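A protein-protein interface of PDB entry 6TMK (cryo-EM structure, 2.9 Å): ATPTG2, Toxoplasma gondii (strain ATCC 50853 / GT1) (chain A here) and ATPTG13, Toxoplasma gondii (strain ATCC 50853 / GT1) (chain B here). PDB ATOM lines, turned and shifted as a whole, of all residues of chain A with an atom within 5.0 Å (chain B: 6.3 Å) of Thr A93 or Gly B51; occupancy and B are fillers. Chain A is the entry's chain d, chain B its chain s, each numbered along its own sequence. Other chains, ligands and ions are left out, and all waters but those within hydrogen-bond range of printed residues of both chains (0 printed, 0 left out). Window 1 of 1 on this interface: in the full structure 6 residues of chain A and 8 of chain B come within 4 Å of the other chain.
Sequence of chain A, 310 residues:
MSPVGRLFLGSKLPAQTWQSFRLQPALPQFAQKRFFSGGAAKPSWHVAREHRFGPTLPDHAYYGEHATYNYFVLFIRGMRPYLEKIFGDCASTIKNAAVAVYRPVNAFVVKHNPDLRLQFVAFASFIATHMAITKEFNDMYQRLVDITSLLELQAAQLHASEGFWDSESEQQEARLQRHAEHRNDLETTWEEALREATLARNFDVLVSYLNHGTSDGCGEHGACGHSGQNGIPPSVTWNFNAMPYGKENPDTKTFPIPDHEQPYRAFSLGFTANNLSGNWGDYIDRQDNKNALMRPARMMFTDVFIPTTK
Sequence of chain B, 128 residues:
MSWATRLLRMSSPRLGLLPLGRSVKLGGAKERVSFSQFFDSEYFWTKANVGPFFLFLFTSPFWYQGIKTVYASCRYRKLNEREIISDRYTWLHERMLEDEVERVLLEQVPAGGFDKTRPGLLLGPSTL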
ATOM      1  N   GLY A  88      -3.981 -21.315  28.494  1.00  0.00           N
ATOM      2  CA  GLY A  88      -3.528 -22.640  28.867  1.00  0.00           C
ATOM      3  C   GLY A  88      -4.681 -23.586  29.125  1.00  0.00           C
ATOM      4  O   GLY A  88      -4.653 -24.743  28.699  1.00  0.00           O
ATOM      5  N   ASP A  89      -5.725 -23.102  29.799  1.00  0.00           N
ATOM      6  CA  ASP A  89      -6.892 -23.938  30.046  1.00  0.00           C
ATOM      7  C   ASP A  89      -7.572 -24.323  28.740  1.00  0.00           C
ATOM      8  O   ASP A  89      -7.943 -25.486  28.540  1.00  0.00           O
ATOM      9  CB  ASP A  89      -7.863 -23.207  30.967  1.00  0.00           C
ATOM     10  CG  ASP A  89      -7.493 -23.346  32.431  1.00  0.00           C
ATOM     11  OD1 ASP A  89      -8.316 -22.975  33.292  1.00  0.00           O
ATOM     12  OD2 ASP A  89      -6.377 -23.822  32.722  1.00  0.00           O
ATOM     13  N   CYS A  90      -7.739 -23.359  27.835  1.00  0.00           N
ATOM     14  CA  CYS A  90      -8.394 -23.646  26.562  1.00  0.00           C
ATOM     15  C   CYS A  90      -7.586 -24.649  25.746  1.00  0.00           C
ATOM     16  O   CYS A  90      -8.136 -25.614  25.193  1.00  0.00           O
ATOM     17  CB  CYS A  90      -8.589 -22.349  25.782  1.00  0.00           C
ATOM     18  SG  CYS A  90      -9.854 -21.259  26.456  1.00  0.00           S
ATOM     19  N   ALA A  91      -6.272 -24.436  25.658  1.00  0.00           N
ATOM     20  CA  ALA A  91      -5.420 -25.347  24.911  1.00  0.00           C
ATOM     21  C   ALA A  91      -5.430 -26.740  25.525  1.00  0.00           C
ATOM     22  O   ALA A  91      -5.443 -27.741  24.802  1.00  0.00           O
ATOM     23  CB  ALA A  91      -4.000 -24.795  24.855  1.00  0.00           C
ATOM     24  N   SER A  92      -5.415 -26.830  26.856  1.00  0.00           N
ATOM     25  CA  SER A  92      -5.455 -28.134  27.504  1.00  0.00           C
ATOM     26  C   SER A  92      -6.771 -28.844  27.225  1.00  0.00           C
ATOM     27  O   SER A  92      -6.792 -30.059  27.002  1.00  0.00           O
ATOM     28  CB  SER A  92      -5.235 -27.974  29.004  1.00  0.00           C
ATOM     29  OG  SER A  92      -3.991 -27.349  29.259  1.00  0.00           O
ATOM     30  N   THR A  93      -7.878 -28.103  27.227  1.00  0.00           N
ATOM     31  CA  THR A  93      -9.170 -28.702  26.913  1.00  0.00           C
ATOM     32  C   THR A  93      -9.162 -29.276  25.502  1.00  0.00           C
ATOM     33  O   THR A  93      -9.553 -30.432  25.279  1.00  0.00           O
ATOM     34  CB  THR A  93     -10.274 -27.657  27.070  1.00  0.00           C
ATOM     35  OG1 THR A  93     -10.387 -27.283  28.446  1.00  0.00           O
ATOM     36  CG2 THR A  93     -11.607 -28.192  26.588  1.00  0.00           C
ATOM     37  N   ILE A  94      -8.703 -28.480  24.537  1.00  0.00           N
ATOM     38  CA  ILE A  94      -8.676 -28.940  23.151  1.00  0.00           C
ATOM     39  C   ILE A  94      -7.763 -30.151  23.010  1.00  0.00           C
ATOM     40  O   ILE A  94      -8.096 -31.122  22.320  1.00  0.00           O
ATOM     41  CB  ILE A  94      -8.243 -27.796  22.221  1.00  0.00           C
ATOM     42  CG1 ILE A  94      -9.305 -26.704  22.204  1.00  0.00           C
ATOM     43  CG2 ILE A  94      -8.013 -28.308  20.818  1.00  0.00           C
ATOM     44  CD1 ILE A  94      -8.794 -25.384  21.725  1.00  0.00           C
ATOM     45  N   LYS A  95      -6.596 -30.108  23.652  1.00  0.00           N
ATOM     46  CA  LYS A  95      -5.643 -31.203  23.543  1.00  0.00           C
ATOM     47  C   LYS A  95      -6.203 -32.481  24.146  1.00  0.00           C
ATOM     48  O   LYS A  95      -6.036 -33.567  23.581  1.00  0.00           O
ATOM     49  CB  LYS A  95      -4.340 -30.824  24.237  1.00  0.00           C
ATOM     50  CG  LYS A  95      -3.366 -31.966  24.379  1.00  0.00           C
ATOM     51  CD  LYS A  95      -1.981 -31.473  24.729  1.00  0.00           C
ATOM     52  CE  LYS A  95      -1.349 -32.344  25.794  1.00  0.00           C
ATOM     53  NZ  LYS A  95       0.071 -31.988  26.039  1.00  0.00           N
ATOM     54  N   ASN A  96      -6.868 -32.375  25.295  1.00  0.00           N
ATOM     55  CA  ASN A  96      -7.439 -33.554  25.926  1.00  0.00           C
ATOM     56  C   ASN A  96      -8.543 -34.150  25.067  1.00  0.00           C
ATOM     57  O   ASN A  96      -8.644 -35.376  24.940  1.00  0.00           O
ATOM     58  CB  ASN A  96      -7.970 -33.193  27.309  1.00  0.00           C
ATOM     59  CG  ASN A  96      -6.873 -32.750  28.252  1.00  0.00           C
ATOM     60  OD1 ASN A  96      -5.721 -33.161  28.120  1.00  0.00           O
ATOM     61  ND2 ASN A  96      -7.225 -31.905  29.213  1.00  0.00           N
ATOM     62  N   ALA A  97      -9.360 -33.303  24.443  1.00  0.00           N
ATOM     63  CA  ALA A  97     -10.395 -33.811  23.548  1.00  0.00           C
ATOM     64  C   ALA A  97      -9.781 -34.527  22.349  1.00  0.00           C
ATOM     65  O   ALA A  97     -10.182 -35.647  21.999  1.00  0.00           O
ATOM     66  CB  ALA A  97     -11.286 -32.663  23.086  1.00  0.00           C
ATOM     67  N   ASN B  49     -11.282 -24.910  35.996  1.00  0.00           N
ATOM     68  CA  ASN B  49     -10.923 -25.068  34.593  1.00  0.00           C
ATOM     69  C   ASN B  49     -11.878 -24.187  33.796  1.00  0.00           C
ATOM     70  O   ASN B  49     -13.050 -24.528  33.615  1.00  0.00           O
ATOM     71  CB  ASN B  49     -11.005 -26.529  34.163  1.00  0.00           C
ATOM     72  CG  ASN B  49     -10.614 -26.733  32.719  1.00  0.00           C
ATOM     73  OD1 ASN B  49      -9.946 -25.893  32.118  1.00  0.00           O
ATOM     74  ND2 ASN B  49     -11.026 -27.857  32.151  1.00  0.00           N
ATOM     75  N   VAL B  50     -11.368 -23.053  33.322  1.00  0.00           N
ATOM     76  CA  VAL B  50     -12.178 -22.057  32.635  1.00  0.00           C
ATOM     77  C   VAL B  50     -12.113 -22.216  31.122  1.00  0.00           C
ATOM     78  O   VAL B  50     -12.589 -21.346  30.386  1.00  0.00           O
ATOM     79  CB  VAL B  50     -11.760 -20.641  33.051  1.00  0.00           C
ATOM     80  CG1 VAL B  50     -12.092 -20.413  34.500  1.00  0.00           C
ATOM     81  CG2 VAL B  50     -10.282 -20.431  32.818  1.00  0.00           C
ATOM     82  N   GLY B  51     -11.555 -23.319  30.642  1.00  0.00           N
ATOM     83  CA  GLY B  51     -11.392 -23.547  29.231  1.00  0.00           C
ATOM     84  C   GLY B  51     -12.711 -23.655  28.504  1.00  0.00           C
ATOM     85  O   GLY B  51     -12.948 -22.971  27.508  1.00  0.00           O
ATOM     86  N   PRO B  52     -13.588 -24.543  28.969  1.00  0.00           N
ATOM     87  CA  PRO B  52     -14.909 -24.647  28.334  1.00  0.00           C
ATOM     88  C   PRO B  52     -15.702 -23.359  28.405  1.00  0.00           C
ATOM     89  O   PRO B  52     -16.357 -22.977  27.427  1.00  0.00           O
ATOM     90  CB  PRO B  52     -15.580 -25.772  29.129  1.00  0.00           C
ATOM     91  CG  PRO B  52     -14.464 -26.569  29.669  1.00  0.00           C
ATOM     92  CD  PRO B  52     -13.390 -25.587  29.984  1.00  0.00           C
ATOM     93  N   PHE B  53     -15.652 -22.669  29.545  1.00  0.00           N
ATOM     94  CA  PHE B  53     -16.363 -21.405  29.677  1.00  0.00           C
ATOM     95  C   PHE B  53     -15.884 -20.399  28.641  1.00  0.00           C
ATOM     96  O   PHE B  53     -16.689 -19.806  27.913  1.00  0.00           O
ATOM     97  CB  PHE B  53     -16.187 -20.851  31.089  1.00  0.00           C
ATOM     98  CG  PHE B  53     -16.764 -19.484  31.276  1.00  0.00           C
ATOM     99  CD1 PHE B  53     -15.947 -18.393  31.484  1.00  0.00           C
ATOM    100  CD2 PHE B  53     -18.130 -19.291  31.233  1.00  0.00           C
ATOM    101  CE1 PHE B  53     -16.482 -17.137  31.649  1.00  0.00           C
ATOM    102  CE2 PHE B  53     -18.668 -18.037  31.399  1.00  0.00           C
ATOM    103  CZ  PHE B  53     -17.842 -16.958  31.607  1.00  0.00           C
ATOM    104  N   PHE B  54     -14.569 -20.205  28.541  1.00  0.00           N
ATOM    105  CA  PHE B  54     -14.059 -19.208  27.611  1.00  0.00           C
ATOM    106  C   PHE B  54     -14.174 -19.652  26.161  1.00  0.00           C
ATOM    107  O   PHE B  54     -14.281 -18.801  25.274  1.00  0.00           O
ATOM    108  CB  PHE B  54     -12.607 -18.881  27.942  1.00  0.00           C
ATOM    109  CG  PHE B  54     -12.456 -17.831  28.996  1.00  0.00           C
ATOM    110  CD1 PHE B  54     -12.667 -16.501  28.699  1.00  0.00           C
ATOM    111  CD2 PHE B  54     -12.118 -18.176  30.287  1.00  0.00           C
ATOM    112  CE1 PHE B  54     -12.537 -15.538  29.667  1.00  0.00           C
ATOM    113  CE2 PHE B  54     -11.988 -17.215  31.259  1.00  0.00           C
ATOM    114  CZ  PHE B  54     -12.194 -15.896  30.950  1.00  0.00           C
ATOM    115  N   LEU B  55     -14.209 -20.956  25.897  1.00  0.00           N
ATOM    116  CA  LEU B  55     -14.444 -21.417  24.535  1.00  0.00           C
ATOM    117  C   LEU B  55     -15.882 -21.155  24.110  1.00  0.00           C
ATOM    118  O   LEU B  55     -16.132 -20.688  22.992  1.00  0.00           O
ATOM    119  CB  LEU B  55     -14.121 -22.902  24.434  1.00  0.00           C
ATOM    120  CG  LEU B  55     -12.641 -23.270  24.389  1.00  0.00           C
ATOM    121  CD1 LEU B  55     -12.468 -24.746  24.625  1.00  0.00           C
ATOM    122  CD2 LEU B  55     -12.027 -22.883  23.073  1.00  0.00           C
ATOM    123  N   PHE B  56     -16.839 -21.462  24.986  1.00  0.00           N
ATOM    124  CA  PHE B  56     -18.219 -21.062  24.753  1.00  0.00           C
ATOM    125  C   PHE B  56     -18.323 -19.559  24.544  1.00  0.00           C
ATOM    126  O   PHE B  56     -19.070 -19.092  23.678  1.00  0.00           O
ATOM    127  CB  PHE B  56     -19.089 -21.504  25.927  1.00  0.00           C
ATOM    128  CG  PHE B  56     -20.528 -21.109  25.798  1.00  0.00           C
ATOM    129  CD1 PHE B  56     -21.392 -21.849  25.013  1.00  0.00           C
ATOM    130  CD2 PHE B  56     -21.019 -20.006  26.469  1.00  0.00           C
ATOM    131  CE1 PHE B  56     -22.716 -21.491  24.891  1.00  0.00           C
ATOM    132  CE2 PHE B  56     -22.344 -19.642  26.352  1.00  0.00           C
ATOM    133  CZ  PHE B  56     -23.194 -20.388  25.562  1.00  0.00           C
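The side-chain carboxylate (OD1) of Asp A89 is in hydrogen-bond range of the backbone NH (N) of Val B50 (3.1 Å). The side-chain sulfur (SG) of Cys A90 lies within hydrogen-bond range of the backbone carbonyl oxygen (O) of Gly B51, at 3.7 Å.
OG1 of Thr A93 sits at hydrogen-bond distance from O of Asp A89 (3.0 Å). The backbone NH (N) of Gly B51 lies close to the side-chain amide oxygen (OD1) of Asn B49 (3.4 Å).
Among the printed residues, merely in contact across the chains: Asp A89 with Asn B49, Asp A89 with Gly B51, Thr A93 with Pro B52, Thr A93 with Asn B49, Cys A90 with Phe B54 and Thr A93 with Gly B51.
Gly B51 touches just these residues of chain A: Asp A89, Cys A90 and Thr A93. Of the printed residues of chain B, Cys A90 touches Gly B51 (3.7 Å) and Phe B54 (3.9 Å). Printed residues of chain A within 4 Å of Phe B54: Cys A90. Printed residues of chain A within 4 Å of Val B50: Asp A89. Ser A92 touches none of the printed residues of chain B. Phe B53 touches none of the printed residues of chain A. The nearest printed residue of chain A that does not touch Gly B51 is Ala A91 (6.3 Å).
Of the 10 printed residues of chain A, 3 touch a printed residue of chain B. Along chain A the printed residues that touch a printed residue of chain B span positions 89 to 93. Of the 8 printed residues of chain B, 5 touch a printed residue of chain A. Hydrophobic or aromatic side chains of chain B within 4 Å of the printed part of chain A: Val B50, Pro B52 and Phe B54. Among the printed residues, 8 pairs touch across the chains. Among the printed residues, no Asp or Glu carboxylate lies within 4 Å of a Lys or Arg side-chain nitrogen of the other chain.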
